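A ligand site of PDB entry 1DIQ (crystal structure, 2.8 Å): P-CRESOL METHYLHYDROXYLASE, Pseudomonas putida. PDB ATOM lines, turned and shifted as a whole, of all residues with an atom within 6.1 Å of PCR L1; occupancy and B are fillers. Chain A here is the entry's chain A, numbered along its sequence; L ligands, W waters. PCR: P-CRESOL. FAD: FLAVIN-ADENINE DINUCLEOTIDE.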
ATOM      1  N   TYR A  95      12.430 -17.144   7.831  1.00  0.00           N
ATOM      2  CA  TYR A  95      12.490 -16.480   9.132  1.00  0.00           C
ATOM      3  C   TYR A  95      13.912 -16.329   9.719  1.00  0.00           C
ATOM      4  O   TYR A  95      14.084 -15.879  10.865  1.00  0.00           O
ATOM      5  CB  TYR A  95      11.550 -17.134  10.166  1.00  0.00           C
ATOM      6  CG  TYR A  95      10.065 -16.838  10.004  1.00  0.00           C
ATOM      7  CD1 TYR A  95       9.586 -15.507   9.960  1.00  0.00           C
ATOM      8  CD2 TYR A  95       9.115 -17.890   9.879  1.00  0.00           C
ATOM      9  CE1 TYR A  95       8.199 -15.216   9.788  1.00  0.00           C
ATOM     10  CE2 TYR A  95       7.713 -17.615   9.710  1.00  0.00           C
ATOM     11  CZ  TYR A  95       7.277 -16.271   9.663  1.00  0.00           C
ATOM     12  OH  TYR A  95       5.940 -15.992   9.487  1.00  0.00           O
ATOM     13  N   ALA A 154       3.925 -26.792   7.903  1.00  0.00           N
ATOM     14  CA  ALA A 154       4.101 -27.502   6.612  1.00  0.00           C
ATOM     15  C   ALA A 154       5.437 -28.242   6.387  1.00  0.00           C
ATOM     16  O   ALA A 154       5.414 -29.277   5.742  1.00  0.00           O
ATOM     17  CB  ALA A 154       3.748 -26.627   5.430  1.00  0.00           C
ATOM     18  N   VAL A 170       2.297 -22.147  13.611  1.00  0.00           N
ATOM     19  CA  VAL A 170       0.948 -22.659  13.408  1.00  0.00           C
ATOM     20  C   VAL A 170       0.784 -23.943  12.593  1.00  0.00           C
ATOM     21  O   VAL A 170       1.518 -24.181  11.619  1.00  0.00           O
ATOM     22  CB  VAL A 170       0.046 -21.572  12.774  1.00  0.00           C
ATOM     23  CG1 VAL A 170      -0.226 -20.461  13.799  1.00  0.00           C
ATOM     24  CG2 VAL A 170       0.693 -20.983  11.518  1.00  0.00           C
ATOM     25  N   TYR A 172      -2.461 -27.114  11.362  1.00  0.00           N
ATOM     26  CA  TYR A 172      -3.752 -27.156  10.667  1.00  0.00           C
ATOM     27  C   TYR A 172      -4.844 -28.061  11.229  1.00  0.00           C
ATOM     28  O   TYR A 172      -5.930 -28.127  10.653  1.00  0.00           O
ATOM     29  CB  TYR A 172      -3.523 -27.483   9.163  1.00  0.00           C
ATOM     30  CG  TYR A 172      -2.567 -26.507   8.517  1.00  0.00           C
ATOM     31  CD1 TYR A 172      -2.981 -25.206   8.195  1.00  0.00           C
ATOM     32  CD2 TYR A 172      -1.185 -26.816   8.436  1.00  0.00           C
ATOM     33  CE1 TYR A 172      -2.048 -24.209   7.837  1.00  0.00           C
ATOM     34  CE2 TYR A 172      -0.237 -25.816   8.069  1.00  0.00           C
ATOM     35  CZ  TYR A 172      -0.687 -24.518   7.777  1.00  0.00           C
ATOM     36  OH  TYR A 172       0.191 -23.512   7.477  1.00  0.00           O
ATOM     37  N   TRP A 285      -0.883 -18.835  -4.511  1.00  0.00           N
ATOM     38  CA  TRP A 285      -0.375 -19.716  -3.448  1.00  0.00           C
ATOM     39  C   TRP A 285      -0.769 -21.132  -3.859  1.00  0.00           C
ATOM     40  O   TRP A 285       0.038 -22.056  -3.783  1.00  0.00           O
ATOM     41  CB  TRP A 285      -0.991 -19.411  -2.071  1.00  0.00           C
ATOM     42  CG  TRP A 285      -0.414 -20.251  -0.897  1.00  0.00           C
ATOM     43  CD1 TRP A 285      -0.554 -21.602  -0.688  1.00  0.00           C
ATOM     44  CD2 TRP A 285       0.400 -19.773   0.178  1.00  0.00           C
ATOM     45  NE1 TRP A 285       0.119 -21.996   0.438  1.00  0.00           N
ATOM     46  CE2 TRP A 285       0.710 -20.893   0.995  1.00  0.00           C
ATOM     47  CE3 TRP A 285       0.877 -18.507   0.553  1.00  0.00           C
ATOM     48  CZ2 TRP A 285       1.501 -20.778   2.172  1.00  0.00           C
ATOM     49  CZ3 TRP A 285       1.668 -18.392   1.730  1.00  0.00           C
ATOM     50  CH2 TRP A 285       1.956 -19.520   2.520  1.00  0.00           C
ATOM     51  N   ARG A 368      -3.172 -30.990   1.729  1.00  0.00           N
ATOM     52  CA  ARG A 368      -3.914 -30.225   2.712  1.00  0.00           C
ATOM     53  C   ARG A 368      -4.689 -31.183   3.618  1.00  0.00           C
ATOM     54  O   ARG A 368      -4.676 -31.034   4.835  1.00  0.00           O
ATOM     55  CB  ARG A 368      -4.824 -29.209   2.031  1.00  0.00           C
ATOM     56  CG  ARG A 368      -4.077 -28.372   1.021  1.00  0.00           C
ATOM     57  CD  ARG A 368      -4.094 -26.853   1.199  1.00  0.00           C
ATOM     58  NE  ARG A 368      -3.273 -26.311   2.272  1.00  0.00           N
ATOM     59  CZ  ARG A 368      -2.693 -25.112   2.274  1.00  0.00           C
ATOM     60  NH1 ARG A 368      -2.801 -24.292   1.232  1.00  0.00           N
ATOM     61  NH2 ARG A 368      -2.089 -24.674   3.366  1.00  0.00           N
ATOM     62  N   GLU A 380       4.228 -28.273   0.022  1.00  0.00           N
ATOM     63  CA  GLU A 380       4.132 -26.816   0.021  1.00  0.00           C
ATOM     64  C   GLU A 380       5.434 -26.102  -0.358  1.00  0.00           C
ATOM     65  O   GLU A 380       5.415 -24.901  -0.613  1.00  0.00           O
ATOM     66  CB  GLU A 380       3.589 -26.284   1.356  1.00  0.00           C
ATOM     67  CG  GLU A 380       2.940 -24.930   1.205  1.00  0.00           C
ATOM     68  CD  GLU A 380       2.203 -24.480   2.425  1.00  0.00           C
ATOM     69  OE1 GLU A 380       0.957 -24.488   2.381  1.00  0.00           O
ATOM     70  OE2 GLU A 380       2.845 -24.067   3.396  1.00  0.00           O
ATOM     71  N   LEU A 383       6.285 -23.600  -3.494  1.00  0.00           N
ATOM     72  CA  LEU A 383       6.174 -22.150  -3.476  1.00  0.00           C
ATOM     73  C   LEU A 383       7.510 -21.508  -3.845  1.00  0.00           C
ATOM     74  O   LEU A 383       7.548 -20.417  -4.405  1.00  0.00           O
ATOM     75  CB  LEU A 383       5.763 -21.652  -2.086  1.00  0.00           C
ATOM     76  CG  LEU A 383       4.340 -21.839  -1.579  1.00  0.00           C
ATOM     77  CD1 LEU A 383       4.284 -21.286  -0.170  1.00  0.00           C
ATOM     78  CD2 LEU A 383       3.340 -21.124  -2.464  1.00  0.00           C
ATOM     79  N   TRP A 394       8.683 -14.153   4.821  1.00  0.00           N
ATOM     80  CA  TRP A 394       7.285 -14.167   5.245  1.00  0.00           C
ATOM     81  C   TRP A 394       6.831 -12.861   5.846  1.00  0.00           C
ATOM     82  O   TRP A 394       7.417 -12.371   6.817  1.00  0.00           O
ATOM     83  CB  TRP A 394       7.017 -15.254   6.254  1.00  0.00           C
ATOM     84  CG  TRP A 394       7.420 -16.602   5.831  1.00  0.00           C
ATOM     85  CD1 TRP A 394       8.482 -17.286   6.267  1.00  0.00           C
ATOM     86  CD2 TRP A 394       6.762 -17.429   4.871  1.00  0.00           C
ATOM     87  NE1 TRP A 394       8.576 -18.507   5.637  1.00  0.00           N
ATOM     88  CE2 TRP A 394       7.524 -18.625   4.770  1.00  0.00           C
ATOM     89  CE3 TRP A 394       5.594 -17.309   4.092  1.00  0.00           C
ATOM     90  CZ2 TRP A 394       7.171 -19.679   3.914  1.00  0.00           C
ATOM     91  CZ3 TRP A 394       5.239 -18.376   3.230  1.00  0.00           C
ATOM     92  CH2 TRP A 394       6.020 -19.535   3.147  1.00  0.00           C
ATOM     93  N   ALA A 396       3.826 -11.570   7.634  1.00  0.00           N
ATOM     94  CA  ALA A 396       2.634 -12.146   8.241  1.00  0.00           C
ATOM     95  C   ALA A 396       1.860 -11.271   9.231  1.00  0.00           C
ATOM     96  O   ALA A 396       1.981 -11.451  10.449  1.00  0.00           O
ATOM     97  CB  ALA A 396       2.963 -13.533   8.840  1.00  0.00           C
ATOM     98  N   GLU A 427      -2.183 -16.485   1.926  1.00  0.00           N
ATOM     99  CA  GLU A 427      -3.230 -17.303   2.510  1.00  0.00           C
ATOM    100  C   GLU A 427      -3.590 -16.796   3.885  1.00  0.00           C
ATOM    101  O   GLU A 427      -2.750 -16.170   4.554  1.00  0.00           O
ATOM    102  CB  GLU A 427      -2.860 -18.796   2.571  1.00  0.00           C
ATOM    103  CG  GLU A 427      -1.755 -19.197   3.534  1.00  0.00           C
ATOM    104  CD  GLU A 427      -1.600 -20.711   3.655  1.00  0.00           C
ATOM    105  OE1 GLU A 427      -2.062 -21.448   2.757  1.00  0.00           O
ATOM    106  OE2 GLU A 427      -0.963 -21.172   4.636  1.00  0.00           O
ATOM    107  N   ILE A 429      -4.891 -17.939   7.579  1.00  0.00           N
ATOM    108  CA  ILE A 429      -5.027 -19.116   8.450  1.00  0.00           C
ATOM    109  C   ILE A 429      -6.035 -18.652   9.510  1.00  0.00           C
ATOM    110  O   ILE A 429      -5.761 -17.733  10.288  1.00  0.00           O
ATOM    111  CB  ILE A 429      -3.690 -19.575   9.061  1.00  0.00           C
ATOM    112  CG1 ILE A 429      -2.650 -19.791   7.956  1.00  0.00           C
ATOM    113  CG2 ILE A 429      -3.937 -20.855   9.911  1.00  0.00           C
ATOM    114  CD1 ILE A 429      -1.298 -20.101   8.451  1.00  0.00           C
ATOM    115  N   HIS A 436      -4.124 -15.230  10.541  1.00  0.00           N
ATOM    116  CA  HIS A 436      -2.684 -15.111  10.380  1.00  0.00           C
ATOM    117  C   HIS A 436      -2.660 -14.883   8.868  1.00  0.00           C
ATOM    118  O   HIS A 436      -2.901 -15.821   8.106  1.00  0.00           O
ATOM    119  CB  HIS A 436      -1.950 -16.414  10.681  1.00  0.00           C
ATOM    120  CG  HIS A 436      -1.572 -16.597  12.108  1.00  0.00           C
ATOM    121  ND1 HIS A 436      -2.466 -17.008  13.073  1.00  0.00           N
ATOM    122  CD2 HIS A 436      -0.371 -16.526  12.714  1.00  0.00           C
ATOM    123  CE1 HIS A 436      -1.822 -17.204  14.205  1.00  0.00           C
ATOM    124  NE2 HIS A 436      -0.542 -16.920  14.017  1.00  0.00           N
ATOM    125  N   VAL A 438      -0.786 -14.722   6.023  1.00  0.00           N
ATOM    126  CA  VAL A 438       0.564 -15.104   5.628  1.00  0.00           C
ATOM    127  C   VAL A 438       0.859 -14.804   4.151  1.00  0.00           C
ATOM    128  O   VAL A 438       0.282 -15.410   3.268  1.00  0.00           O
ATOM    129  CB  VAL A 438       0.807 -16.608   5.934  1.00  0.00           C
ATOM    130  CG1 VAL A 438       2.202 -17.035   5.541  1.00  0.00           C
ATOM    131  CG2 VAL A 438       0.581 -16.870   7.398  1.00  0.00           C
ATOM    132  N   TYR A 473       3.231 -10.995  13.499  1.00  0.00           N
ATOM    133  CA  TYR A 473       3.313 -11.880  14.664  1.00  0.00           C
ATOM    134  C   TYR A 473       4.655 -12.591  14.832  1.00  0.00           C
ATOM    135  O   TYR A 473       4.902 -13.234  15.853  1.00  0.00           O
ATOM    136  CB  TYR A 473       2.171 -12.923  14.580  1.00  0.00           C
ATOM    137  CG  TYR A 473       2.516 -14.254  13.908  1.00  0.00           C
ATOM    138  CD1 TYR A 473       2.683 -15.441  14.686  1.00  0.00           C
ATOM    139  CD2 TYR A 473       2.737 -14.331  12.524  1.00  0.00           C
ATOM    140  CE1 TYR A 473       3.060 -16.675  14.083  1.00  0.00           C
ATOM    141  CE2 TYR A 473       3.121 -15.563  11.900  1.00  0.00           C
ATOM    142  CZ  TYR A 473       3.269 -16.729  12.688  1.00  0.00           C
ATOM    143  OH  TYR A 473       3.615 -17.919  12.084  1.00  0.00           O
ATOM    144  N   ARG A 474       5.443 -12.568  13.764  1.00  0.00           N
ATOM    145  CA  ARG A 474       6.737 -13.243  13.691  1.00  0.00           C
ATOM    146  C   ARG A 474       7.435 -12.645  12.453  1.00  0.00           C
ATOM    147  O   ARG A 474       6.774 -12.280  11.480  1.00  0.00           O
ATOM    148  CB  ARG A 474       6.465 -14.730  13.462  1.00  0.00           C
ATOM    149  CG  ARG A 474       7.572 -15.714  13.611  1.00  0.00           C
ATOM    150  CD  ARG A 474       6.950 -17.080  13.392  1.00  0.00           C
ATOM    151  NE  ARG A 474       7.909 -18.163  13.242  1.00  0.00           N
ATOM    152  CZ  ARG A 474       7.605 -19.396  12.824  1.00  0.00           C
ATOM    153  NH1 ARG A 474       6.353 -19.709  12.499  1.00  0.00           N
ATOM    154  NH2 ARG A 474       8.561 -20.301  12.715  1.00  0.00           N
HETATM  155  CB  PCR L   1       2.381 -21.896   5.435  1.00  0.00           C
HETATM  156  CG  PCR L   1       2.938 -20.875   6.395  1.00  0.00           C
HETATM  157  CD1 PCR L   1       2.224 -20.540   7.572  1.00  0.00           C
HETATM  158  CE1 PCR L   1       2.737 -19.599   8.525  1.00  0.00           C
HETATM  159  CD2 PCR L   1       4.197 -20.242   6.175  1.00  0.00           C
HETATM  160  CE2 PCR L   1       4.731 -19.304   7.116  1.00  0.00           C
HETATM  161  CZ  PCR L   1       3.980 -18.972   8.290  1.00  0.00           C
HETATM  162  OH  PCR L   1       4.417 -18.011   9.172  1.00  0.00           O
HETATM  163  PA  FAD L   2      13.884 -23.830  14.642  1.00  0.00           P
HETATM  164  O1A FAD L   2      14.656 -24.929  15.232  1.00  0.00           O
HETATM  165  O2A FAD L   2      14.394 -23.189  13.439  1.00  0.00           O
HETATM  166  O5B FAD L   2      13.655 -22.796  15.832  1.00  0.00           O
HETATM  167  C5B FAD L   2      12.917 -21.594  15.493  1.00  0.00           C
HETATM  168  C4B FAD L   2      13.371 -20.463  16.346  1.00  0.00           C
HETATM  169  O4B FAD L   2      13.059 -20.785  17.711  1.00  0.00           O
HETATM  170  C3B FAD L   2      14.882 -20.292  16.369  1.00  0.00           C
HETATM  171  O3B FAD L   2      15.383 -19.555  15.312  1.00  0.00           O
HETATM  172  C2B FAD L   2      15.152 -19.596  17.638  1.00  0.00           C
HETATM  173  O2B FAD L   2      15.080 -18.179  17.585  1.00  0.00           O
HETATM  174  C1B FAD L   2      14.122 -20.278  18.555  1.00  0.00           C
HETATM  175  N9A FAD L   2      14.870 -21.355  19.300  1.00  0.00           N
HETATM  176  C8A FAD L   2      14.904 -22.684  18.826  1.00  0.00           C
HETATM  177  N7A FAD L   2      15.094 -23.590  19.686  1.00  0.00           N
HETATM  178  C5A FAD L   2      15.178 -22.896  20.869  1.00  0.00           C
HETATM  179  C6A FAD L   2      15.458 -23.329  22.215  1.00  0.00           C
HETATM  180  N6A FAD L   2      15.681 -24.616  22.470  1.00  0.00           N
HETATM  181  N1A FAD L   2      15.496 -22.384  23.218  1.00  0.00           N
HETATM  182  C2A FAD L   2      15.266 -21.085  22.891  1.00  0.00           C
HETATM  183  N3A FAD L   2      15.004 -20.553  21.648  1.00  0.00           N
HETATM  184  C4A FAD L   2      14.991 -21.545  20.669  1.00  0.00           C
HETATM  185  N1  FAD L   2       5.739 -22.277   9.812  1.00  0.00           N
HETATM  186  C2  FAD L   2       4.651 -22.411  10.558  1.00  0.00           C
HETATM  187  O2  FAD L   2       4.571 -22.059  11.736  1.00  0.00           O
HETATM  188  N3  FAD L   2       3.594 -23.003   9.885  1.00  0.00           N
HETATM  189  C4  FAD L   2       3.583 -23.536   8.582  1.00  0.00           C
HETATM  190  O4  FAD L   2       2.567 -24.103   8.222  1.00  0.00           O
HETATM  191  C4X FAD L   2       4.761 -23.285   7.818  1.00  0.00           C
HETATM  192  N5  FAD L   2       4.727 -23.694   6.475  1.00  0.00           N
HETATM  193  C5X FAD L   2       5.894 -23.421   5.799  1.00  0.00           C
HETATM  194  C6  FAD L   2       5.927 -23.792   4.411  1.00  0.00           C
HETATM  195  C7  FAD L   2       7.057 -23.596   3.641  1.00  0.00           C
HETATM  196  C7M FAD L   2       7.066 -23.983   2.210  1.00  0.00           C
HETATM  197  C8  FAD L   2       8.221 -22.991   4.247  1.00  0.00           C
HETATM  198  C8M FAD L   2       9.445 -22.773   3.525  1.00  0.00           C
HETATM  199  C9  FAD L   2       8.214 -22.627   5.545  1.00  0.00           C
HETATM  200  C9A FAD L   2       7.072 -22.814   6.363  1.00  0.00           C
HETATM  201  N10 FAD L   2       7.004 -22.433   7.755  1.00  0.00           N
HETATM  202  C10 FAD L   2       5.792 -22.665   8.504  1.00  0.00           C
HETATM  203  C1' FAD L   2       8.149 -21.821   8.464  1.00  0.00           C
HETATM  204  C2' FAD L   2       8.722 -23.069   9.241  1.00  0.00           C
HETATM  205  O2' FAD L   2       9.969 -23.393   8.670  1.00  0.00           O
HETATM  206  C3' FAD L   2       8.761 -22.836  10.767  1.00  0.00           C
HETATM  207  O3' FAD L   2       7.527 -22.579  11.329  1.00  0.00           O
HETATM  208  C4' FAD L   2       9.222 -23.945  11.706  1.00  0.00           C
HETATM  209  O4' FAD L   2       9.011 -25.324  11.421  1.00  0.00           O
HETATM  210  C5' FAD L   2      10.586 -23.510  12.049  1.00  0.00           C
HETATM  211  O5' FAD L   2      11.374 -24.607  12.030  1.00  0.00           O
HETATM  212  P   FAD L   2      11.925 -25.296  13.287  1.00  0.00           P
HETATM  213  O1P FAD L   2      13.109 -26.032  12.781  1.00  0.00           O
HETATM  214  O2P FAD L   2      10.815 -26.038  13.828  1.00  0.00           O
HETATM  215  O3P FAD L   2      12.395 -24.306  14.396  1.00  0.00           O
HETATM  216  O   HOH W   1      -0.346 -23.632   4.696  1.00  0.00           O
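The guanidinium group (NH2) of Arg 368 is in salt-bridge range of the side-chain carboxylate (OE1) of Glu 380, 3.2 Å away.
The backbone carbonyl oxygen (O) of Glu 427 sits at hydrogen-bond distance from the backbone NH (N) of Val 438 (2.8 Å).
The side-chain carboxylate (OE1) of Glu 427 lies within salt-bridge range of the guanidinium group (NH2) of Arg 368 (3.3 Å).
The backbone NH (N) of Tyr 473 sits at hydrogen-bond distance from the backbone carbonyl oxygen (O) of Ala 396 (3.3 Å).
The backbone NH of Ile 429 sits at hydrogen-bond distance from the backbone carbonyl oxygen of His 436 (3.0 Å).
OE1 of Glu 427 lies within hydrogen-bond range of NE1 of Trp 285 (3.2 Å).
The side-chain carboxylate of Glu 380 is in hydrogen-bond range of the indole nitrogen of Trp 285 (3.3 Å).
NH1 of Arg 474 sits at hydrogen-bond distance from OH of Tyr 473, at 3.3 Å.
The backbone NH of Val 170 lies within hydrogen-bond range of an oxygen (O2) of FAD L2.
An oxygen (O4) of FAD L2 lies within hydrogen-bond range of the side-chain hydroxyl (OH) of Tyr 172.
An oxygen (O4) of FAD L2 sits at hydrogen-bond distance from the backbone NH of Ala 154 (3.0 Å).
The backbone carbonyl oxygen of Val 170 sits at hydrogen-bond distance from a nitrogen (N3) of FAD L2 (3.0 Å).
The guanidinium group (NH2) of Arg 474 is in hydrogen-bond range of an oxygen (O3') of FAD L2, 2.9 Å away.
OH of Tyr 473 is in hydrogen-bond range of OH of PCR L1 (3.0 Å).
OH of Tyr 95 sits at hydrogen-bond distance from OH of PCR L1.
Residues that only touch PCR L1: Val 170, Tyr 172, Trp 285, Glu 380, Trp 394, Glu 427, Ile 429 and Val 438.
Ten residues have an atom within 4 Å of PCR L1: Tyr 95, Val 170, Tyr 172, Trp 285, Glu 380, Trp 394, Glu 427, Ile 429, Val 438 and Tyr 473.
Water W1 lies within hydrogen-bond range of the guanidinium group (NH2) of Arg 368, the side-chain carboxylate (OE2) of Glu 427, the side-chain carboxylate (OE1) of Glu 380 and the side-chain hydroxyl (OH) of Tyr 172.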
